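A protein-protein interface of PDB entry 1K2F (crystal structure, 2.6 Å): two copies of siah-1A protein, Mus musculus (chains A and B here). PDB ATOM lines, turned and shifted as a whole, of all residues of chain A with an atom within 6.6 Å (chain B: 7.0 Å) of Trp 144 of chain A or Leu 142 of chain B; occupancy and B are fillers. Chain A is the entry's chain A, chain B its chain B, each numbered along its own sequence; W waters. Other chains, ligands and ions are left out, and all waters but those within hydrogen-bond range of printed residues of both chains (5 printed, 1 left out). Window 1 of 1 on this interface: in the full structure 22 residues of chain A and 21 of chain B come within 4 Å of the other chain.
O of Thr 143 of chain B is in hydrogen-bond range of N of Thr 143 of chain A, at 2.8 Å.
NH1 of Arg 141 of chain B is in salt-bridge range of OE2 of Glu 145 of chain A, 2.9 Å away.
The side-chain hydroxyl (OG1) of Thr 147 of chain A lies within hydrogen-bond range of the guanidinium group (NH1) of Arg 139 of chain B (3.5 Å).
The side-chain carboxylate (OD2) of Asp 163 of chain A lies within salt-bridge range of the guanidinium group (NH2) of Arg 140 of chain B.
The side-chain hydroxyl of Tyr 131 of chain A is in hydrogen-bond range of the indole nitrogen of Trp 144 of chain A (3.1 Å).
The backbone carbonyl oxygen (O) of Trp 144 of chain A sits at hydrogen-bond distance from the backbone NH (N) of Leu 133 of chain A, 2.8 Å away.
The backbone NH of Leu 135 of chain B lies within hydrogen-bond range of the backbone carbonyl oxygen of Leu 142 of chain B (2.9 Å).
Among the printed residues, pairs that only touch across the chains: Leu 142 of chain A with Thr 143 of chain B (3.4 Å), Thr 143 of chain A with Arg 141 of chain B (3.6 Å), Thr 143 of chain A with Leu 142 of chain B (3.5 Å), Trp 144 of chain A with Arg 141 of chain B (3.5 Å), Trp 144 of chain A with Leu 142 of chain B (3.8 Å), Trp 144 of chain A with Phe 175 of chain B (3.95 Å), Glu 145 of chain A with Arg 140 of chain B (3.1 Å), Ala 146 of chain A with Arg 139 of chain B (3.5 Å), Ser 162 of chain A with Ile 171 of chain B (3.5 Å), Ser 162 of chain A with Leu 174 of chain B (3.5 Å), Asp 163 of chain A with Leu 174 of chain B (3.7 Å) and Val 166 of chain A with Ile 171 of chain B (3.8 Å).
Of chain B, only Arg 141 (3.5 Å), Leu 142 (3.8 Å) and Phe 175 (3.95 Å) come within 4 Å of Trp 144 of chain A.
Of chain A, only Thr 143 and Trp 144 come within 4 Å of Leu 142 of chain B.
Of the printed residues of chain B, Ala 146 of chain A touches Arg 139 (3.5 Å).
Of the printed residues of chain A, Arg 141 of chain B touches Thr 143, Trp 144 and Glu 145.
Of the printed residues of chain B, Leu 142 of chain A touches Thr 143 (3.4 Å).
Of the printed residues of chain A, Arg 140 of chain B touches Glu 145 (3.1 Å) and Asp 163 (3.1 Å).
Val 166 of chain B touches none of the printed residues of chain A.
The nearest residue of chain B that does not touch Trp 144 of chain A is Arg 140 of chain B (4.2 Å).
The nearest residue of chain A that does not touch Leu 142 of chain B is Leu 142 of chain A (4.4 Å).
The nearest printed residue of chain B that does not touch Thr 143 of chain A is Trp 144 of chain B (5.0 Å).
Hydrophobic or aromatic side chains of chain B that line the printed part of chain A: Leu 142, Ile 171, Leu 174 and Phe 175.
Of the 17 printed residues of chain A, 9 touch a printed residue of chain B.
Hydrophobic or aromatic side chains of chain A within 4 Å of the printed part of chain B: Leu 142, Trp 144, Ala 146 and Val 166.
Among the printed residues, Asp or Glu carboxylates within 4 Å of a Lys or Arg side-chain nitrogen of the other chain: Glu 145 of chain A with Arg 141 of chain B (2.9 Å) and Asp 163 of chain A with Arg 140 of chain B (3.1 Å).
Leu 142 of chain A touches Thr 143 of chain B, and with the chains exchanged Thr 143 of chain A touches Leu 142 of chain B.
Thr 143 of chain B touches its own counterpart, Thr 143 of chain A.
Trp 144 of chain A touches Leu 142 of chain B, but with the chains exchanged Leu 142 of chain A does not touch Trp 144 of chain B (4.2 Å).
Of the 16 pairs that touch across the chains among the printed residues, 3 have their exchanged pair printed and touching as well.
Water W1 lies within hydrogen-bond range of the backbone carbonyl oxygen of Val 166 of chain A (2.7 Å) and the backbone carbonyl oxygen of Val 166 of chain B (2.9 Å).
Water W2 bridges the side-chain carboxylate (OE2) of Glu 145 of chain A and the guanidinium group (NH1) of Arg 141 of chain B.
Water W5 lies within hydrogen-bond range of the side-chain hydroxyl (OG1) of Thr 143 of chain A (3.0 Å) and the backbone carbonyl oxygen (O) of Thr 143 of chain B (3.3 Å).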
ATOM      1  N   ALA A 115      22.916 -36.734  -0.933  1.00  0.00           N
ATOM      2  CA  ALA A 115      24.369 -36.856  -1.029  1.00  0.00           C
ATOM      3  C   ALA A 115      24.970 -35.995   0.066  1.00  0.00           C
ATOM      4  O   ALA A 115      24.656 -34.805   0.162  1.00  0.00           O
ATOM      5  CB  ALA A 115      24.862 -36.384  -2.389  1.00  0.00           C
ATOM      6  N   ILE A 116      25.851 -36.584   0.866  1.00  0.00           N
ATOM      7  CA  ILE A 116      26.488 -35.869   1.975  1.00  0.00           C
ATOM      8  C   ILE A 116      27.905 -36.398   2.225  1.00  0.00           C
ATOM      9  O   ILE A 116      28.242 -37.504   1.804  1.00  0.00           O
ATOM     10  CB  ILE A 116      25.622 -36.023   3.252  1.00  0.00           C
ATOM     11  CG1 ILE A 116      26.138 -35.133   4.379  1.00  0.00           C
ATOM     12  CG2 ILE A 116      25.543 -37.491   3.670  1.00  0.00           C
ATOM     13  CD1 ILE A 116      25.207 -35.064   5.579  1.00  0.00           C
ATOM     14  N   TYR A 131      33.225 -28.951   2.071  1.00  0.00           N
ATOM     15  CA  TYR A 131      33.122 -29.797   0.890  1.00  0.00           C
ATOM     16  C   TYR A 131      32.161 -29.230  -0.137  1.00  0.00           C
ATOM     17  O   TYR A 131      31.261 -28.472   0.200  1.00  0.00           O
ATOM     18  CB  TYR A 131      32.716 -31.225   1.270  1.00  0.00           C
ATOM     19  CG  TYR A 131      31.262 -31.413   1.634  1.00  0.00           C
ATOM     20  CD1 TYR A 131      30.388 -32.058   0.759  1.00  0.00           C
ATOM     21  CD2 TYR A 131      30.767 -30.994   2.860  1.00  0.00           C
ATOM     22  CE1 TYR A 131      29.067 -32.285   1.101  1.00  0.00           C
ATOM     23  CE2 TYR A 131      29.441 -31.215   3.211  1.00  0.00           C
ATOM     24  CZ  TYR A 131      28.600 -31.862   2.326  1.00  0.00           C
ATOM     25  OH  TYR A 131      27.292 -32.092   2.664  1.00  0.00           O
ATOM     26  N   ARG A 132      32.379 -29.588  -1.395  1.00  0.00           N
ATOM     27  CA  ARG A 132      31.534 -29.132  -2.486  1.00  0.00           C
ATOM     28  C   ARG A 132      31.162 -30.330  -3.338  1.00  0.00           C
ATOM     29  O   ARG A 132      32.026 -31.143  -3.655  1.00  0.00           O
ATOM     30  CB  ARG A 132      32.269 -28.102  -3.346  1.00  0.00           C
ATOM     31  CG  ARG A 132      31.480 -27.652  -4.568  1.00  0.00           C
ATOM     32  CD  ARG A 132      32.213 -26.585  -5.358  1.00  0.00           C
ATOM     33  NE  ARG A 132      33.363 -27.127  -6.070  1.00  0.00           N
ATOM     34  CZ  ARG A 132      34.375 -26.400  -6.538  1.00  0.00           C
ATOM     35  NH1 ARG A 132      34.393 -25.082  -6.372  1.00  0.00           N
ATOM     36  NH2 ARG A 132      35.378 -26.999  -7.170  1.00  0.00           N
ATOM     37  N   LEU A 133      29.870 -30.459  -3.645  1.00  0.00           N
ATOM     38  CA  LEU A 133      29.364 -31.538  -4.477  1.00  0.00           C
ATOM     39  C   LEU A 133      28.801 -30.944  -5.760  1.00  0.00           C
ATOM     40  O   LEU A 133      28.034 -29.982  -5.710  1.00  0.00           O
ATOM     41  CB  LEU A 133      28.266 -32.319  -3.755  1.00  0.00           C
ATOM     42  CG  LEU A 133      28.684 -33.045  -2.478  1.00  0.00           C
ATOM     43  CD1 LEU A 133      27.514 -33.844  -1.920  1.00  0.00           C
ATOM     44  CD2 LEU A 133      29.862 -33.948  -2.756  1.00  0.00           C
ATOM     45  N   GLU A 134      29.200 -31.489  -6.907  1.00  0.00           N
ATOM     46  CA  GLU A 134      28.701 -30.993  -8.185  1.00  0.00           C
ATOM     47  C   GLU A 134      28.137 -32.054  -9.104  1.00  0.00           C
ATOM     48  O   GLU A 134      28.671 -33.150  -9.208  1.00  0.00           O
ATOM     49  CB  GLU A 134      29.788 -30.242  -8.974  1.00  0.00           C
ATOM     50  CG  GLU A 134      30.167 -28.873  -8.459  1.00  0.00           C
ATOM     51  CD  GLU A 134      31.096 -28.116  -9.412  1.00  0.00           C
ATOM     52  OE1 GLU A 134      31.302 -28.569 -10.567  1.00  0.00           O
ATOM     53  OE2 GLU A 134      31.619 -27.051  -9.007  1.00  0.00           O
ATOM     54  N   LEU A 142      24.388 -28.249 -10.803  1.00  0.00           N
ATOM     55  CA  LEU A 142      23.757 -28.240  -9.488  1.00  0.00           C
ATOM     56  C   LEU A 142      24.873 -28.427  -8.470  1.00  0.00           C
ATOM     57  O   LEU A 142      25.547 -29.467  -8.446  1.00  0.00           O
ATOM     58  CB  LEU A 142      22.742 -29.372  -9.356  1.00  0.00           C
ATOM     59  CG  LEU A 142      22.004 -29.403  -8.013  1.00  0.00           C
ATOM     60  CD1 LEU A 142      21.289 -28.088  -7.790  1.00  0.00           C
ATOM     61  CD2 LEU A 142      21.028 -30.570  -7.966  1.00  0.00           C
ATOM     62  N   THR A 143      25.040 -27.428  -7.609  1.00  0.00           N
ATOM     63  CA  THR A 143      26.105 -27.442  -6.614  1.00  0.00           C
ATOM     64  C   THR A 143      25.659 -27.279  -5.169  1.00  0.00           C
ATOM     65  O   THR A 143      24.786 -26.464  -4.864  1.00  0.00           O
ATOM     66  CB  THR A 143      27.124 -26.326  -6.920  1.00  0.00           C
ATOM     67  OG1 THR A 143      27.654 -26.531  -8.228  1.00  0.00           O
ATOM     68  CG2 THR A 143      28.275 -26.335  -5.931  1.00  0.00           C
ATOM     69  N   TRP A 144      26.313 -28.031  -4.286  1.00  0.00           N
ATOM     70  CA  TRP A 144      26.052 -27.972  -2.859  1.00  0.00           C
ATOM     71  C   TRP A 144      27.384 -27.799  -2.116  1.00  0.00           C
ATOM     72  O   TRP A 144      28.312 -28.596  -2.302  1.00  0.00           O
ATOM     73  CB  TRP A 144      25.333 -29.250  -2.391  1.00  0.00           C
ATOM     74  CG  TRP A 144      25.194 -29.354  -0.886  1.00  0.00           C
ATOM     75  CD1 TRP A 144      25.985 -30.080  -0.047  1.00  0.00           C
ATOM     76  CD2 TRP A 144      24.263 -28.656  -0.052  1.00  0.00           C
ATOM     77  NE1 TRP A 144      25.621 -29.869   1.252  1.00  0.00           N
ATOM     78  CE2 TRP A 144      24.567 -29.000   1.285  1.00  0.00           C
ATOM     79  CE3 TRP A 144      23.208 -27.767  -0.301  1.00  0.00           C
ATOM     80  CZ2 TRP A 144      23.854 -28.483   2.382  1.00  0.00           C
ATOM     81  CZ3 TRP A 144      22.496 -27.245   0.791  1.00  0.00           C
ATOM     82  CH2 TRP A 144      22.828 -27.608   2.118  1.00  0.00           C
ATOM     83  N   GLU A 145      27.475 -26.754  -1.294  1.00  0.00           N
ATOM     84  CA  GLU A 145      28.677 -26.480  -0.499  1.00  0.00           C
ATOM     85  C   GLU A 145      28.284 -26.410   0.959  1.00  0.00           C
ATOM     86  O   GLU A 145      27.325 -25.720   1.302  1.00  0.00           O
ATOM     87  CB  GLU A 145      29.308 -25.141  -0.891  1.00  0.00           C
ATOM     88  CG  GLU A 145      30.050 -25.146  -2.205  1.00  0.00           C
ATOM     89  CD  GLU A 145      30.251 -23.757  -2.761  1.00  0.00           C
ATOM     90  OE1 GLU A 145      31.352 -23.196  -2.603  1.00  0.00           O
ATOM     91  OE2 GLU A 145      29.297 -23.218  -3.357  1.00  0.00           O
ATOM     92  N   ALA A 146      29.045 -27.083   1.819  1.00  0.00           N
ATOM     93  CA  ALA A 146      28.753 -27.092   3.252  1.00  0.00           C
ATOM     94  C   ALA A 146      29.893 -27.679   4.078  1.00  0.00           C
ATOM     95  O   ALA A 146      30.897 -28.124   3.532  1.00  0.00           O
ATOM     96  CB  ALA A 146      27.474 -27.874   3.514  1.00  0.00           C
ATOM     97  N   THR A 147      29.718 -27.682   5.394  1.00  0.00           N
ATOM     98  CA  THR A 147      30.704 -28.228   6.310  1.00  0.00           C
ATOM     99  C   THR A 147      30.424 -29.709   6.485  1.00  0.00           C
ATOM    100  O   THR A 147      29.284 -30.105   6.724  1.00  0.00           O
ATOM    101  CB  THR A 147      30.622 -27.562   7.700  1.00  0.00           C
ATOM    102  OG1 THR A 147      30.725 -26.144   7.556  1.00  0.00           O
ATOM    103  CG2 THR A 147      31.746 -28.053   8.594  1.00  0.00           C
ATOM    104  N   SER A 162      17.356 -32.583   5.488  1.00  0.00           N
ATOM    105  CA  SER A 162      17.720 -32.156   4.135  1.00  0.00           C
ATOM    106  C   SER A 162      18.937 -31.221   4.099  1.00  0.00           C
ATOM    107  O   SER A 162      19.059 -30.396   3.199  1.00  0.00           O
ATOM    108  CB  SER A 162      16.530 -31.487   3.432  1.00  0.00           C
ATOM    109  OG  SER A 162      15.570 -32.439   3.003  1.00  0.00           O
ATOM    110  N   ASP A 163      19.813 -31.338   5.097  1.00  0.00           N
ATOM    111  CA  ASP A 163      21.022 -30.529   5.164  1.00  0.00           C
ATOM    112  C   ASP A 163      22.115 -31.253   4.386  1.00  0.00           C
ATOM    113  O   ASP A 163      23.064 -31.804   4.967  1.00  0.00           O
ATOM    114  CB  ASP A 163      21.453 -30.340   6.612  1.00  0.00           C
ATOM    115  CG  ASP A 163      22.237 -29.057   6.829  1.00  0.00           C
ATOM    116  OD1 ASP A 163      22.561 -28.374   5.836  1.00  0.00           O
ATOM    117  OD2 ASP A 163      22.518 -28.723   8.003  1.00  0.00           O
ATOM    118  N   CYS A 164      21.959 -31.251   3.065  1.00  0.00           N
ATOM    119  CA  CYS A 164      22.886 -31.913   2.154  1.00  0.00           C
ATOM    120  C   CYS A 164      22.366 -31.708   0.732  1.00  0.00           C
ATOM    121  O   CYS A 164      21.429 -30.946   0.510  1.00  0.00           O
ATOM    122  CB  CYS A 164      22.944 -33.417   2.462  1.00  0.00           C
ATOM    123  SG  CYS A 164      21.350 -34.282   2.235  1.00  0.00           S
ATOM    124  N   LEU A 165      22.975 -32.368  -0.236  1.00  0.00           N
ATOM    125  CA  LEU A 165      22.489 -32.240  -1.600  1.00  0.00           C
ATOM    126  C   LEU A 165      21.217 -33.092  -1.747  1.00  0.00           C
ATOM    127  O   LEU A 165      21.234 -34.291  -1.475  1.00  0.00           O
ATOM    128  CB  LEU A 165      23.550 -32.709  -2.597  1.00  0.00           C
ATOM    129  CG  LEU A 165      23.071 -32.624  -4.041  1.00  0.00           C
ATOM    130  CD1 LEU A 165      22.641 -31.202  -4.349  1.00  0.00           C
ATOM    131  CD2 LEU A 165      24.143 -33.116  -4.990  1.00  0.00           C
ATOM    132  N   VAL A 166      20.111 -32.470  -2.145  1.00  0.00           N
ATOM    133  CA  VAL A 166      18.864 -33.211  -2.315  1.00  0.00           C
ATOM    134  C   VAL A 166      18.318 -33.063  -3.723  1.00  0.00           C
ATOM    135  O   VAL A 166      18.059 -31.956  -4.183  1.00  0.00           O
ATOM    136  CB  VAL A 166      17.748 -32.779  -1.296  1.00  0.00           C
ATOM    137  CG1 VAL A 166      16.461 -33.585  -1.522  1.00  0.00           C
ATOM    138  CG2 VAL A 166      18.216 -32.988   0.127  1.00  0.00           C
ATOM    139  N   LEU B 133      21.499 -19.234  -9.918  1.00  0.00           N
ATOM    140  CA  LEU B 133      20.643 -18.982  -8.769  1.00  0.00           C
ATOM    141  C   LEU B 133      21.356 -19.477  -7.534  1.00  0.00           C
ATOM    142  O   LEU B 133      21.833 -20.612  -7.508  1.00  0.00           O
ATOM    143  CB  LEU B 133      19.327 -19.749  -8.876  1.00  0.00           C
ATOM    144  CG  LEU B 133      18.415 -19.474 -10.057  1.00  0.00           C
ATOM    145  CD1 LEU B 133      17.124 -20.273  -9.871  1.00  0.00           C
ATOM    146  CD2 LEU B 133      18.136 -17.990 -10.130  1.00  0.00           C
ATOM    147  N   GLU B 134      21.409 -18.646  -6.504  1.00  0.00           N
ATOM    148  CA  GLU B 134      22.061 -19.042  -5.269  1.00  0.00           C
ATOM    149  C   GLU B 134      21.221 -18.858  -4.035  1.00  0.00           C
ATOM    150  O   GLU B 134      20.485 -17.887  -3.913  1.00  0.00           O
ATOM    151  CB  GLU B 134      23.357 -18.268  -5.048  1.00  0.00           C
ATOM    152  CG  GLU B 134      24.548 -18.719  -5.862  1.00  0.00           C
ATOM    153  CD  GLU B 134      25.841 -18.081  -5.384  1.00  0.00           C
ATOM    154  OE1 GLU B 134      25.790 -16.962  -4.827  1.00  0.00           O
ATOM    155  OE2 GLU B 134      26.910 -18.704  -5.547  1.00  0.00           O
ATOM    156  N   LEU B 135      21.291 -19.842  -3.150  1.00  0.00           N
ATOM    157  CA  LEU B 135      20.629 -19.774  -1.859  1.00  0.00           C
ATOM    158  C   LEU B 135      21.855 -19.718  -0.957  1.00  0.00           C
ATOM    159  O   LEU B 135      22.653 -20.662  -0.917  1.00  0.00           O
ATOM    160  CB  LEU B 135      19.803 -21.026  -1.549  1.00  0.00           C
ATOM    161  CG  LEU B 135      18.579 -21.385  -2.400  1.00  0.00           C
ATOM    162  CD1 LEU B 135      17.664 -22.305  -1.595  1.00  0.00           C
ATOM    163  CD2 LEU B 135      17.806 -20.150  -2.810  1.00  0.00           C
ATOM    164  N   ASN B 136      22.082 -18.563  -0.346  1.00  0.00           N
ATOM    165  CA  ASN B 136      23.224 -18.399   0.531  1.00  0.00           C
ATOM    166  C   ASN B 136      22.873 -18.414   1.998  1.00  0.00           C
ATOM    167  O   ASN B 136      21.957 -17.729   2.448  1.00  0.00           O
ATOM    168  CB  ASN B 136      24.006 -17.140   0.173  1.00  0.00           C
ATOM    169  CG  ASN B 136      25.228 -17.449  -0.666  1.00  0.00           C
ATOM    170  OD1 ASN B 136      26.189 -18.039  -0.170  1.00  0.00           O
ATOM    171  ND2 ASN B 136      25.180 -17.104  -1.951  1.00  0.00           N
ATOM    172  N   GLY B 137      23.614 -19.218   2.741  1.00  0.00           N
ATOM    173  CA  GLY B 137      23.370 -19.313   4.163  1.00  0.00           C
ATOM    174  C   GLY B 137      24.662 -19.302   4.938  1.00  0.00           C
ATOM    175  O   GLY B 137      25.729 -19.034   4.394  1.00  0.00           O
ATOM    176  N   ARG B 139      27.562 -20.943   6.291  1.00  0.00           N
ATOM    177  CA  ARG B 139      28.361 -22.146   6.052  1.00  0.00           C
ATOM    178  C   ARG B 139      27.673 -23.188   5.143  1.00  0.00           C
ATOM    179  O   ARG B 139      27.808 -24.406   5.340  1.00  0.00           O
ATOM    180  CB  ARG B 139      28.788 -22.775   7.392  1.00  0.00           C
ATOM    181  CG  ARG B 139      29.579 -21.836   8.298  1.00  0.00           C
ATOM    182  CD  ARG B 139      30.960 -22.390   8.641  1.00  0.00           C
ATOM    183  NE  ARG B 139      31.016 -23.059   9.942  1.00  0.00           N
ATOM    184  CZ  ARG B 139      31.964 -23.927  10.302  1.00  0.00           C
ATOM    185  NH1 ARG B 139      32.947 -24.256   9.460  1.00  0.00           N
ATOM    186  NH2 ARG B 139      31.957 -24.437  11.526  1.00  0.00           N
ATOM    187  N   ARG B 140      26.916 -22.693   4.164  1.00  0.00           N
ATOM    188  CA  ARG B 140      26.227 -23.553   3.197  1.00  0.00           C
ATOM    189  C   ARG B 140      25.660 -22.767   2.025  1.00  0.00           C
ATOM    190  O   ARG B 140      25.220 -21.628   2.186  1.00  0.00           O
ATOM    191  CB  ARG B 140      25.154 -24.441   3.850  1.00  0.00           C
ATOM    192  CG  ARG B 140      24.044 -23.721   4.553  1.00  0.00           C
ATOM    193  CD  ARG B 140      23.003 -24.713   5.088  1.00  0.00           C
ATOM    194  NE  ARG B 140      23.416 -25.382   6.318  1.00  0.00           N
ATOM    195  CZ  ARG B 140      22.870 -25.155   7.511  1.00  0.00           C
ATOM    196  NH1 ARG B 140      21.885 -24.272   7.638  1.00  0.00           N
ATOM    197  NH2 ARG B 140      23.302 -25.809   8.582  1.00  0.00           N
ATOM    198  N   ARG B 141      25.705 -23.387   0.845  1.00  0.00           N
ATOM    199  CA  ARG B 141      25.235 -22.775  -0.389  1.00  0.00           C
ATOM    200  C   ARG B 141      24.665 -23.775  -1.387  1.00  0.00           C
ATOM    201  O   ARG B 141      25.281 -24.803  -1.661  1.00  0.00           O
ATOM    202  CB  ARG B 141      26.386 -22.024  -1.068  1.00  0.00           C
ATOM    203  CG  ARG B 141      25.967 -21.289  -2.331  1.00  0.00           C
ATOM    204  CD  ARG B 141      27.151 -20.700  -3.066  1.00  0.00           C
ATOM    205  NE  ARG B 141      27.865 -19.736  -2.245  1.00  0.00           N
ATOM    206  CZ  ARG B 141      29.187 -19.636  -2.192  1.00  0.00           C
ATOM    207  NH1 ARG B 141      29.945 -20.441  -2.922  1.00  0.00           N
ATOM    208  NH2 ARG B 141      29.745 -18.765  -1.366  1.00  0.00           N
ATOM    209  N   LEU B 142      23.498 -23.449  -1.940  1.00  0.00           N
ATOM    210  CA  LEU B 142      22.835 -24.286  -2.940  1.00  0.00           C
ATOM    211  C   LEU B 142      22.793 -23.468  -4.223  1.00  0.00           C
ATOM    212  O   LEU B 142      22.168 -22.408  -4.266  1.00  0.00           O
ATOM    213  CB  LEU B 142      21.415 -24.646  -2.505  1.00  0.00           C
ATOM    214  CG  LEU B 142      20.663 -25.587  -3.451  1.00  0.00           C
ATOM    215  CD1 LEU B 142      21.385 -26.925  -3.535  1.00  0.00           C
ATOM    216  CD2 LEU B 142      19.218 -25.775  -2.998  1.00  0.00           C
ATOM    217  N   THR B 143      23.466 -23.953  -5.265  1.00  0.00           N
ATOM    218  CA  THR B 143      23.519 -23.228  -6.530  1.00  0.00           C
ATOM    219  C   THR B 143      23.054 -24.012  -7.762  1.00  0.00           C
ATOM    220  O   THR B 143      23.301 -25.214  -7.898  1.00  0.00           O
ATOM    221  CB  THR B 143      24.952 -22.692  -6.801  1.00  0.00           C
ATOM    222  OG1 THR B 143      25.439 -22.012  -5.643  1.00  0.00           O
ATOM    223  CG2 THR B 143      24.938 -21.704  -7.941  1.00  0.00           C
ATOM    224  N   TRP B 144      22.403 -23.294  -8.666  1.00  0.00           N
ATOM    225  CA  TRP B 144      21.909 -23.857  -9.917  1.00  0.00           C
ATOM    226  C   TRP B 144      22.319 -22.943 -11.074  1.00  0.00           C
ATOM    227  O   TRP B 144      22.083 -21.729 -11.042  1.00  0.00           O
ATOM    228  CB  TRP B 144      20.383 -23.995  -9.881  1.00  0.00           C
ATOM    229  CG  TRP B 144      19.752 -24.259 -11.222  1.00  0.00           C
ATOM    230  CD1 TRP B 144      19.110 -23.355 -12.009  1.00  0.00           C
ATOM    231  CD2 TRP B 144      19.692 -25.512 -11.919  1.00  0.00           C
ATOM    232  NE1 TRP B 144      18.654 -23.959 -13.154  1.00  0.00           N
ATOM    233  CE2 TRP B 144      18.998 -25.288 -13.122  1.00  0.00           C
ATOM    234  CE3 TRP B 144      20.156 -26.803 -11.643  1.00  0.00           C
ATOM    235  CZ2 TRP B 144      18.753 -26.306 -14.050  1.00  0.00           C
ATOM    236  CZ3 TRP B 144      19.915 -27.820 -12.572  1.00  0.00           C
ATOM    237  CH2 TRP B 144      19.218 -27.559 -13.758  1.00  0.00           C
ATOM    238  N   LEU B 165      16.032 -25.001 -10.509  1.00  0.00           N
ATOM    239  CA  LEU B 165      16.461 -25.229  -9.128  1.00  0.00           C
ATOM    240  C   LEU B 165      15.272 -25.823  -8.376  1.00  0.00           C
ATOM    241  O   LEU B 165      14.164 -25.295  -8.447  1.00  0.00           O
ATOM    242  CB  LEU B 165      16.899 -23.925  -8.463  1.00  0.00           C
ATOM    243  CG  LEU B 165      17.149 -23.980  -6.950  1.00  0.00           C
ATOM    244  CD1 LEU B 165      18.156 -25.065  -6.610  1.00  0.00           C
ATOM    245  CD2 LEU B 165      17.643 -22.627  -6.451  1.00  0.00           C
ATOM    246  N   VAL B 166      15.483 -26.956  -7.712  1.00  0.00           N
ATOM    247  CA  VAL B 166      14.404 -27.582  -6.962  1.00  0.00           C
ATOM    248  C   VAL B 166      14.757 -27.843  -5.513  1.00  0.00           C
ATOM    249  O   VAL B 166      15.740 -28.525  -5.217  1.00  0.00           O
ATOM    250  CB  VAL B 166      13.959 -28.928  -7.566  1.00  0.00           C
ATOM    251  CG1 VAL B 166      12.716 -29.418  -6.846  1.00  0.00           C
ATOM    252  CG2 VAL B 166      13.706 -28.799  -9.050  1.00  0.00           C
ATOM    253  N   PHE B 167      13.953 -27.284  -4.614  1.00  0.00           N
ATOM    254  CA  PHE B 167      14.122 -27.490  -3.177  1.00  0.00           C
ATOM    255  C   PHE B 167      12.749 -27.582  -2.517  1.00  0.00           C
ATOM    256  O   PHE B 167      11.731 -27.578  -3.202  1.00  0.00           O
ATOM    257  CB  PHE B 167      15.002 -26.410  -2.524  1.00  0.00           C
ATOM    258  CG  PHE B 167      14.530 -25.001  -2.741  1.00  0.00           C
ATOM    259  CD1 PHE B 167      14.027 -24.255  -1.682  1.00  0.00           C
ATOM    260  CD2 PHE B 167      14.647 -24.393  -3.990  1.00  0.00           C
ATOM    261  CE1 PHE B 167      13.656 -22.934  -1.860  1.00  0.00           C
ATOM    262  CE2 PHE B 167      14.276 -23.067  -4.176  1.00  0.00           C
ATOM    263  CZ  PHE B 167      13.780 -22.336  -3.111  1.00  0.00           C
ATOM    264  N   ILE B 171      14.546 -27.683   3.145  1.00  0.00           N
ATOM    265  CA  ILE B 171      15.759 -27.050   2.652  1.00  0.00           C
ATOM    266  C   ILE B 171      15.649 -25.531   2.810  1.00  0.00           C
ATOM    267  O   ILE B 171      16.615 -24.864   3.207  1.00  0.00           O
ATOM    268  CB  ILE B 171      16.013 -27.425   1.184  1.00  0.00           C
ATOM    269  CG1 ILE B 171      16.275 -28.933   1.077  1.00  0.00           C
ATOM    270  CG2 ILE B 171      17.183 -26.610   0.620  1.00  0.00           C
ATOM    271  CD1 ILE B 171      16.039 -29.510  -0.304  1.00  0.00           C
ATOM    272  N   LEU B 174      16.688 -24.103   6.116  1.00  0.00           N
ATOM    273  CA  LEU B 174      18.118 -23.932   6.353  1.00  0.00           C
ATOM    274  C   LEU B 174      18.649 -22.602   5.838  1.00  0.00           C
ATOM    275  O   LEU B 174      19.748 -22.178   6.217  1.00  0.00           O
ATOM    276  CB  LEU B 174      18.892 -25.044   5.656  1.00  0.00           C
ATOM    277  CG  LEU B 174      18.484 -26.439   6.103  1.00  0.00           C
ATOM    278  CD1 LEU B 174      19.032 -27.466   5.104  1.00  0.00           C
ATOM    279  CD2 LEU B 174      18.968 -26.688   7.552  1.00  0.00           C
ATOM    280  N   PHE B 175      17.893 -21.974   4.939  1.00  0.00           N
ATOM    281  CA  PHE B 175      18.321 -20.716   4.345  1.00  0.00           C
ATOM    282  C   PHE B 175      17.515 -19.495   4.736  1.00  0.00           C
ATOM    283  O   PHE B 175      18.074 -18.418   4.889  1.00  0.00           O
ATOM    284  CB  PHE B 175      18.351 -20.832   2.820  1.00  0.00           C
ATOM    285  CG  PHE B 175      19.401 -21.756   2.312  1.00  0.00           C
ATOM    286  CD1 PHE B 175      19.111 -23.094   2.071  1.00  0.00           C
ATOM    287  CD2 PHE B 175      20.701 -21.300   2.100  1.00  0.00           C
ATOM    288  CE1 PHE B 175      20.102 -23.969   1.631  1.00  0.00           C
ATOM    289  CE2 PHE B 175      21.700 -22.167   1.661  1.00  0.00           C
ATOM    290  CZ  PHE B 175      21.400 -23.502   1.427  1.00  0.00           C
HETATM  291  O   HOH W   1      16.986 -30.832  -6.358  1.00  0.00           O
HETATM  292  O   HOH W   2      29.184 -21.619  -5.780  1.00  0.00           O
HETATM  293  O   HOH W   3      27.317 -26.756   6.808  1.00  0.00           O
HETATM  294  O   HOH W   4      18.622 -29.167  -4.748  1.00  0.00           O
HETATM  295  O   HOH W   5      25.905 -24.608  -9.756  1.00  0.00           O
